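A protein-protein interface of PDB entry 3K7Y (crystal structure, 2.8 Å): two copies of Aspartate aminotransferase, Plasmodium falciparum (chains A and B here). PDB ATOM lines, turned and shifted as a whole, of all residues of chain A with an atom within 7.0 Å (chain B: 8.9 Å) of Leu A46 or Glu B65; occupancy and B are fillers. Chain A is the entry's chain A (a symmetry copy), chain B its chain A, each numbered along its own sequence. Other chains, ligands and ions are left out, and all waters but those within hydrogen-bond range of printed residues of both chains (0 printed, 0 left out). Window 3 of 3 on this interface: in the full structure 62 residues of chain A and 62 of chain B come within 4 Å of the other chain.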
ATOM      1  N   VAL A  38      15.154  11.128 -12.621  1.00  0.00           N
ATOM      2  CA  VAL A  38      13.765  11.063 -13.095  1.00  0.00           C
ATOM      3  C   VAL A  38      13.275  12.392 -13.661  1.00  0.00           C
ATOM      4  O   VAL A  38      13.881  13.439 -13.432  1.00  0.00           O
ATOM      5  CB  VAL A  38      12.782  10.557 -11.986  1.00  0.00           C
ATOM      6  CG1 VAL A  38      13.385   9.400 -11.228  1.00  0.00           C
ATOM      7  CG2 VAL A  38      12.388  11.674 -11.022  1.00  0.00           C
ATOM      8  N   CYS A  39      12.173  12.333 -14.398  1.00  0.00           N
ATOM      9  CA  CYS A  39      11.558  13.521 -14.956  1.00  0.00           C
ATOM     10  C   CYS A  39      10.260  13.854 -14.206  1.00  0.00           C
ATOM     11  O   CYS A  39       9.384  12.994 -14.055  1.00  0.00           O
ATOM     12  CB  CYS A  39      11.326  13.311 -16.450  1.00  0.00           C
ATOM     13  SG  CYS A  39       9.857  14.082 -17.094  1.00  0.00           S
ATOM     14  N   CYS A  40      10.150  15.098 -13.730  1.00  0.00           N
ATOM     15  CA  CYS A  40       9.021  15.533 -12.880  1.00  0.00           C
ATOM     16  C   CYS A  40       7.845  16.139 -13.647  1.00  0.00           C
ATOM     17  O   CYS A  40       8.021  16.789 -14.678  1.00  0.00           O
ATOM     18  CB  CYS A  40       9.489  16.500 -11.781  1.00  0.00           C
ATOM     19  SG  CYS A  40      10.251  15.688 -10.328  1.00  0.00           S
ATOM     20  N   ASN A  41       6.645  15.916 -13.115  1.00  0.00           N
ATOM     21  CA  ASN A  41       5.397  16.450 -13.664  1.00  0.00           C
ATOM     22  C   ASN A  41       5.260  17.960 -13.375  1.00  0.00           C
ATOM     23  O   ASN A  41       6.202  18.586 -12.876  1.00  0.00           O
ATOM     24  CB  ASN A  41       4.215  15.668 -13.067  1.00  0.00           C
ATOM     25  CG  ASN A  41       3.015  15.584 -13.998  1.00  0.00           C
ATOM     26  OD1 ASN A  41       2.047  14.891 -13.689  1.00  0.00           O
ATOM     27  ND2 ASN A  41       3.064  16.281 -15.134  1.00  0.00           N
ATOM     28  N   ASP A  43       3.252  19.090 -11.145  1.00  0.00           N
ATOM     29  CA  ASP A  43       3.118  19.089  -9.683  1.00  0.00           C
ATOM     30  C   ASP A  43       4.393  18.627  -8.973  1.00  0.00           C
ATOM     31  O   ASP A  43       4.359  18.300  -7.782  1.00  0.00           O
ATOM     32  CB  ASP A  43       1.939  18.206  -9.227  1.00  0.00           C
ATOM     33  CG  ASP A  43       0.626  18.572  -9.894  1.00  0.00           C
ATOM     34  OD1 ASP A  43       0.456  19.738 -10.321  1.00  0.00           O
ATOM     35  OD2 ASP A  43      -0.244  17.680  -9.981  1.00  0.00           O
ATOM     36  N   GLY A  44       5.502  18.589  -9.704  1.00  0.00           N
ATOM     37  CA  GLY A  44       6.793  18.213  -9.130  1.00  0.00           C
ATOM     38  C   GLY A  44       6.867  16.792  -8.594  1.00  0.00           C
ATOM     39  O   GLY A  44       7.739  16.477  -7.784  1.00  0.00           O
ATOM     40  N   ASP A  45       5.951  15.937  -9.039  1.00  0.00           N
ATOM     41  CA  ASP A  45       5.974  14.511  -8.704  1.00  0.00           C
ATOM     42  C   ASP A  45       6.142  13.681  -9.978  1.00  0.00           C
ATOM     43  O   ASP A  45       5.851  14.171 -11.075  1.00  0.00           O
ATOM     44  CB  ASP A  45       4.700  14.103  -7.955  1.00  0.00           C
ATOM     45  CG  ASP A  45       3.436  14.624  -8.617  1.00  0.00           C
ATOM     46  OD1 ASP A  45       2.338  14.282  -8.126  1.00  0.00           O
ATOM     47  OD2 ASP A  45       3.538  15.380  -9.616  1.00  0.00           O
ATOM     48  N   LEU A  46       6.590  12.432  -9.829  1.00  0.00           N
ATOM     49  CA  LEU A  46       6.996  11.599 -10.970  1.00  0.00           C
ATOM     50  C   LEU A  46       5.994  11.538 -12.123  1.00  0.00           C
ATOM     51  O   LEU A  46       4.779  11.522 -11.914  1.00  0.00           O
ATOM     52  CB  LEU A  46       7.332  10.180 -10.512  1.00  0.00           C
ATOM     53  CG  LEU A  46       7.779   9.233 -11.634  1.00  0.00           C
ATOM     54  CD1 LEU A  46       9.181   9.586 -12.103  1.00  0.00           C
ATOM     55  CD2 LEU A  46       7.685   7.768 -11.216  1.00  0.00           C
ATOM     56  N   HIS A  47       6.530  11.481 -13.337  1.00  0.00           N
ATOM     57  CA  HIS A  47       5.718  11.466 -14.545  1.00  0.00           C
ATOM     58  C   HIS A  47       5.229  10.074 -14.937  1.00  0.00           C
ATOM     59  O   HIS A  47       5.852   9.064 -14.584  1.00  0.00           O
ATOM     60  CB  HIS A  47       6.500  12.062 -15.716  1.00  0.00           C
ATOM     61  CG  HIS A  47       5.732  12.082 -17.000  1.00  0.00           C
ATOM     62  ND1 HIS A  47       6.137  11.392 -18.120  1.00  0.00           N
ATOM     63  CD2 HIS A  47       4.562  12.685 -17.331  1.00  0.00           C
ATOM     64  CE1 HIS A  47       5.267  11.590 -19.095  1.00  0.00           C
ATOM     65  NE2 HIS A  47       4.302  12.372 -18.641  1.00  0.00           N
ATOM     66  N   ILE A  48       4.108  10.034 -15.665  1.00  0.00           N
ATOM     67  CA  ILE A  48       3.658   8.819 -16.354  1.00  0.00           C
ATOM     68  C   ILE A  48       2.636   9.100 -17.460  1.00  0.00           C
ATOM     69  O   ILE A  48       1.710   9.868 -17.264  1.00  0.00           O
ATOM     70  CB  ILE A  48       3.158   7.705 -15.360  1.00  0.00           C
ATOM     71  CG1 ILE A  48       3.087   6.335 -16.070  1.00  0.00           C
ATOM     72  CG2 ILE A  48       1.846   8.121 -14.649  1.00  0.00           C
ATOM     73  CD1 ILE A  48       3.833   5.240 -15.367  1.00  0.00           C
ATOM     74  N   LEU A  53      -0.287   3.631 -19.049  1.00  0.00           N
ATOM     75  CA  LEU A  53      -1.349   3.151 -18.163  1.00  0.00           C
ATOM     76  C   LEU A  53      -2.345   2.246 -18.904  1.00  0.00           C
ATOM     77  O   LEU A  53      -2.912   1.320 -18.316  1.00  0.00           O
ATOM     78  CB  LEU A  53      -2.096   4.314 -17.488  1.00  0.00           C
ATOM     79  CG  LEU A  53      -1.424   5.299 -16.518  1.00  0.00           C
ATOM     80  CD1 LEU A  53      -2.458   5.980 -15.631  1.00  0.00           C
ATOM     81  CD2 LEU A  53      -0.375   4.641 -15.651  1.00  0.00           C
ATOM     82  N   SER A 252       8.495   6.505 -19.571  1.00  0.00           N
ATOM     83  CA  SER A 252       8.384   6.767 -18.133  1.00  0.00           C
ATOM     84  C   SER A 252       8.348   5.474 -17.299  1.00  0.00           C
ATOM     85  O   SER A 252       7.784   5.471 -16.200  1.00  0.00           O
ATOM     86  CB  SER A 252       7.136   7.595 -17.832  1.00  0.00           C
ATOM     87  OG  SER A 252       6.021   6.720 -17.655  1.00  0.00           O
ATOM     88  N   TYR A 254      10.224   3.650 -15.149  1.00  0.00           N
ATOM     89  CA  TYR A 254      11.430   3.693 -14.356  1.00  0.00           C
ATOM     90  C   TYR A 254      11.697   2.350 -13.668  1.00  0.00           C
ATOM     91  O   TYR A 254      12.608   1.603 -14.068  1.00  0.00           O
ATOM     92  CB  TYR A 254      11.383   4.875 -13.394  1.00  0.00           C
ATOM     93  CG  TYR A 254      11.355   6.214 -14.127  1.00  0.00           C
ATOM     94  CD1 TYR A 254      12.539   6.847 -14.513  1.00  0.00           C
ATOM     95  CD2 TYR A 254      10.154   6.838 -14.444  1.00  0.00           C
ATOM     96  CE1 TYR A 254      12.517   8.067 -15.187  1.00  0.00           C
ATOM     97  CE2 TYR A 254      10.126   8.045 -15.111  1.00  0.00           C
ATOM     98  CZ  TYR A 254      11.306   8.659 -15.478  1.00  0.00           C
ATOM     99  OH  TYR A 254      11.266   9.868 -16.144  1.00  0.00           O
ATOM    100  N   GLY A 255      10.872   2.016 -12.682  1.00  0.00           N
ATOM    101  CA  GLY A 255      11.054   0.787 -11.915  1.00  0.00           C
ATOM    102  C   GLY A 255      10.828  -0.508 -12.671  1.00  0.00           C
ATOM    103  O   GLY A 255      11.202  -1.571 -12.186  1.00  0.00           O
ATOM    104  N   GLU A 256      10.209  -0.438 -13.845  1.00  0.00           N
ATOM    105  CA  GLU A 256       9.951  -1.639 -14.623  1.00  0.00           C
ATOM    106  C   GLU A 256      11.256  -2.253 -15.131  1.00  0.00           C
ATOM    107  O   GLU A 256      11.325  -3.449 -15.446  1.00  0.00           O
ATOM    108  CB  GLU A 256       9.023  -1.306 -15.784  1.00  0.00           C
ATOM    109  CG  GLU A 256       7.547  -1.713 -15.639  1.00  0.00           C
ATOM    110  CD  GLU A 256       7.117  -2.096 -14.226  1.00  0.00           C
ATOM    111  OE1 GLU A 256       7.521  -3.180 -13.736  1.00  0.00           O
ATOM    112  OE2 GLU A 256       6.330  -1.333 -13.629  1.00  0.00           O
ATOM    113  N   VAL B  59      -3.200  -4.996  -8.561  1.00  0.00           N
ATOM    114  CA  VAL B  59      -2.019  -4.149  -8.724  1.00  0.00           C
ATOM    115  C   VAL B  59      -2.188  -3.028  -9.740  1.00  0.00           C
ATOM    116  O   VAL B  59      -1.675  -1.930  -9.552  1.00  0.00           O
ATOM    117  CB  VAL B  59      -0.766  -4.978  -9.052  1.00  0.00           C
ATOM    118  CG1 VAL B  59       0.300  -4.127  -9.733  1.00  0.00           C
ATOM    119  CG2 VAL B  59      -0.223  -5.597  -7.781  1.00  0.00           C
ATOM    120  N   ASN B  62      -4.279  -0.088  -7.958  1.00  0.00           N
ATOM    121  CA  ASN B  62      -3.844   0.669  -6.795  1.00  0.00           C
ATOM    122  C   ASN B  62      -2.625   1.524  -7.067  1.00  0.00           C
ATOM    123  O   ASN B  62      -2.166   2.284  -6.204  1.00  0.00           O
ATOM    124  CB  ASN B  62      -3.583  -0.294  -5.643  1.00  0.00           C
ATOM    125  CG  ASN B  62      -4.840  -1.010  -5.198  1.00  0.00           C
ATOM    126  OD1 ASN B  62      -5.585  -1.555  -6.018  1.00  0.00           O
ATOM    127  ND2 ASN B  62      -5.100  -0.993  -3.894  1.00  0.00           N
ATOM    128  N   TYR B  63      -2.123   1.408  -8.290  1.00  0.00           N
ATOM    129  CA  TYR B  63      -0.836   1.961  -8.643  1.00  0.00           C
ATOM    130  C   TYR B  63      -0.869   2.563 -10.039  1.00  0.00           C
ATOM    131  O   TYR B  63      -1.312   1.913 -10.989  1.00  0.00           O
ATOM    132  CB  TYR B  63       0.206   0.854  -8.603  1.00  0.00           C
ATOM    133  CG  TYR B  63       0.423   0.189  -7.249  1.00  0.00           C
ATOM    134  CD1 TYR B  63       0.970   0.899  -6.174  1.00  0.00           C
ATOM    135  CD2 TYR B  63       0.131  -1.168  -7.060  1.00  0.00           C
ATOM    136  CE1 TYR B  63       1.199   0.283  -4.948  1.00  0.00           C
ATOM    137  CE2 TYR B  63       0.354  -1.790  -5.835  1.00  0.00           C
ATOM    138  CZ  TYR B  63       0.888  -1.058  -4.788  1.00  0.00           C
ATOM    139  OH  TYR B  63       1.118  -1.667  -3.581  1.00  0.00           O
ATOM    140  N   LYS B  64      -0.386   3.797 -10.166  1.00  0.00           N
ATOM    141  CA  LYS B  64      -0.340   4.470 -11.459  1.00  0.00           C
ATOM    142  C   LYS B  64       1.069   4.956 -11.820  1.00  0.00           C
ATOM    143  O   LYS B  64       1.470   4.942 -12.986  1.00  0.00           O
ATOM    144  CB  LYS B  64      -1.386   5.602 -11.542  1.00  0.00           C
ATOM    145  CG  LYS B  64      -1.485   6.535 -10.314  1.00  0.00           C
ATOM    146  CD  LYS B  64      -2.529   6.057  -9.271  1.00  0.00           C
ATOM    147  CE  LYS B  64      -2.196   6.570  -7.856  1.00  0.00           C
ATOM    148  NZ  LYS B  64      -0.837   6.115  -7.355  1.00  0.00           N
ATOM    149  N   GLU B  65       1.820   5.374 -10.809  1.00  0.00           N
ATOM    150  CA  GLU B  65       3.226   5.742 -10.973  1.00  0.00           C
ATOM    151  C   GLU B  65       4.142   4.516 -10.966  1.00  0.00           C
ATOM    152  O   GLU B  65       3.831   3.512 -10.323  1.00  0.00           O
ATOM    153  CB  GLU B  65       3.636   6.634  -9.823  1.00  0.00           C
ATOM    154  CG  GLU B  65       3.355   8.089 -10.022  1.00  0.00           C
ATOM    155  CD  GLU B  65       4.019   8.933  -8.944  1.00  0.00           C
ATOM    156  OE1 GLU B  65       4.836   8.387  -8.159  1.00  0.00           O
ATOM    157  OE2 GLU B  65       3.722  10.149  -8.881  1.00  0.00           O
ATOM    158  N   LYS B  66       5.278   4.605 -11.661  1.00  0.00           N
ATOM    159  CA  LYS B  66       6.276   3.521 -11.661  1.00  0.00           C
ATOM    160  C   LYS B  66       7.704   3.996 -11.342  1.00  0.00           C
ATOM    161  O   LYS B  66       8.516   4.151 -12.242  1.00  0.00           O
ATOM    162  CB  LYS B  66       6.241   2.769 -12.989  1.00  0.00           C
ATOM    163  CG  LYS B  66       4.890   2.166 -13.304  1.00  0.00           C
ATOM    164  CD  LYS B  66       4.856   1.524 -14.683  1.00  0.00           C
ATOM    165  CE  LYS B  66       3.419   1.366 -15.180  1.00  0.00           C
ATOM    166  NZ  LYS B  66       3.325   0.647 -16.486  1.00  0.00           N
ATOM    167  N   PRO B  67       8.012   4.215 -10.049  1.00  0.00           N
ATOM    168  CA  PRO B  67       9.329   4.680  -9.595  1.00  0.00           C
ATOM    169  C   PRO B  67      10.435   3.613  -9.508  1.00  0.00           C
ATOM    170  O   PRO B  67      10.154   2.424  -9.315  1.00  0.00           O
ATOM    171  CB  PRO B  67       9.045   5.212  -8.184  1.00  0.00           C
ATOM    172  CG  PRO B  67       7.568   5.198  -8.036  1.00  0.00           C
ATOM    173  CD  PRO B  67       7.064   4.150  -8.929  1.00  0.00           C
ATOM    174  N   TYR B  68      11.678   4.063  -9.657  1.00  0.00           N
ATOM    175  CA  TYR B  68      12.858   3.291  -9.318  1.00  0.00           C
ATOM    176  C   TYR B  68      12.797   2.859  -7.852  1.00  0.00           C
ATOM    177  O   TYR B  68      12.456   3.678  -6.986  1.00  0.00           O
ATOM    178  CB  TYR B  68      14.096   4.174  -9.444  1.00  0.00           C
ATOM    179  CG  TYR B  68      14.613   4.472 -10.818  1.00  0.00           C
ATOM    180  CD1 TYR B  68      14.724   3.478 -11.777  1.00  0.00           C
ATOM    181  CD2 TYR B  68      15.055   5.753 -11.145  1.00  0.00           C
ATOM    182  CE1 TYR B  68      15.234   3.758 -13.047  1.00  0.00           C
ATOM    183  CE2 TYR B  68      15.567   6.047 -12.415  1.00  0.00           C
ATOM    184  CZ  TYR B  68      15.656   5.037 -13.355  1.00  0.00           C
ATOM    185  OH  TYR B  68      16.165   5.283 -14.605  1.00  0.00           O
ATOM    186  N   ILE B 291       9.648  -3.165 -10.230  1.00  0.00           N
ATOM    187  CA  ILE B 291       8.650  -2.616  -9.333  1.00  0.00           C
ATOM    188  C   ILE B 291       7.323  -3.379  -9.456  1.00  0.00           C
ATOM    189  O   ILE B 291       6.656  -3.633  -8.456  1.00  0.00           O
ATOM    190  CB  ILE B 291       8.538  -1.082  -9.534  1.00  0.00           C
ATOM    191  CG1 ILE B 291       8.161  -0.368  -8.223  1.00  0.00           C
ATOM    192  CG2 ILE B 291       7.713  -0.737 -10.761  1.00  0.00           C
ATOM    193  CD1 ILE B 291       6.882   0.387  -8.241  1.00  0.00           C
ATOM    194  N   HIS B 292       6.979  -3.798 -10.670  1.00  0.00           N
ATOM    195  CA  HIS B 292       5.761  -4.574 -10.887  1.00  0.00           C
ATOM    196  C   HIS B 292       5.744  -5.845 -10.067  1.00  0.00           C
ATOM    197  O   HIS B 292       4.792  -6.106  -9.338  1.00  0.00           O
ATOM    198  CB  HIS B 292       5.580  -4.928 -12.362  1.00  0.00           C
ATOM    199  CG  HIS B 292       4.588  -6.025 -12.601  1.00  0.00           C
ATOM    200  ND1 HIS B 292       3.230  -5.799 -12.685  1.00  0.00           N
ATOM    201  CD2 HIS B 292       4.760  -7.361 -12.767  1.00  0.00           C
ATOM    202  CE1 HIS B 292       2.609  -6.941 -12.911  1.00  0.00           C
ATOM    203  NE2 HIS B 292       3.514  -7.905 -12.961  1.00  0.00           N
ATOM    204  N   ARG B 295       5.266  -5.168  -6.433  1.00  0.00           N
ATOM    205  CA  ARG B 295       3.849  -4.911  -6.145  1.00  0.00           C
ATOM    206  C   ARG B 295       2.959  -6.176  -6.171  1.00  0.00           C
ATOM    207  O   ARG B 295       2.233  -6.423  -5.211  1.00  0.00           O
ATOM    208  CB  ARG B 295       3.296  -3.825  -7.077  1.00  0.00           C
ATOM    209  CG  ARG B 295       3.924  -2.438  -6.859  1.00  0.00           C
ATOM    210  CD  ARG B 295       3.596  -1.452  -7.988  1.00  0.00           C
ATOM    211  NE  ARG B 295       3.860  -0.069  -7.587  1.00  0.00           N
ATOM    212  CZ  ARG B 295       3.752   0.994  -8.384  1.00  0.00           C
ATOM    213  NH1 ARG B 295       3.391   0.859  -9.652  1.00  0.00           N
ATOM    214  NH2 ARG B 295       4.011   2.206  -7.907  1.00  0.00           N
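Leu A46 touches just these residues of chain B: Glu B65, Lys B66 and Pro B67. Of the printed residues of chain B, Ile A48 touches Lys B64 and Lys B66. Of the printed residues of chain B, Tyr A254 touches Lys B66 and Tyr B68. Of the printed residues of chain A, His B292 touches Glu A256 (3.0 Å). Arg B295 touches none of the printed residues of chain A. Tyr B63 touches none of the printed residues of chain A. The nearest residue of chain A that does not touch Glu B65 is Asp A45 (4.2 Å). The nearest printed residue of chain B that does not touch Tyr A254 is Pro B67 (4.2 Å).
No position is printed for both chains.
The guanidinium group (NH2) of Arg B295 is in hydrogen-bond range of the backbone carbonyl oxygen (O) of Glu B65, at 2.8 Å. The backbone NH of Cys A39 is in hydrogen-bond range of the side-chain hydroxyl of Tyr A254 (3.2 Å).
Among the printed residues, pairs that only touch across the chains: Leu A46 with Lys B66 (3.8 Å), Leu A46 with Pro B67 (3.8 Å), Ile A48 with Lys B64 (3.4 Å), Ile A48 with Lys B66 (3.9 Å), Leu A53 with Lys B64 (3.3 Å), Tyr A254 with Tyr B68 (3.5 Å), Gly A255 with Tyr B68 (3.7 Å), Glu A256 with Lys B66 (3.4 Å) and Glu A256 with Ile B291 (3.2 Å).
N of Gly A255 sits close to O of Pro B67, at 3.5 Å. O of Lys B66 is in hydrogen-bond range of N of Gly A255, at 3.2 Å. The backbone NH of Tyr A254 lies close to the backbone carbonyl oxygen of Lys B66, 3.4 Å away. The backbone carbonyl oxygen (O) of Leu A46 sits close to the side-chain carboxylate (OE2) of Glu B65 (3.5 Å). The backbone NH (N) of His B292 sits close to the side-chain carboxylate (OE1) of Glu A256 (3.2 Å). The backbone NH (N) of Ile B291 lies within hydrogen-bond range of the backbone carbonyl oxygen (O) of Gly A255.
Of the 11 printed residues of chain B, 7 touch a printed residue of chain A. Hydrophobic or aromatic side chains of chain A within 4 Å of the printed part of chain B: Leu A46, Ile A48, Leu A53 and Tyr A254. Among the printed residues, no Asp or Glu carboxylate lies within 4 Å of a Lys or Arg side-chain nitrogen of the other chain.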
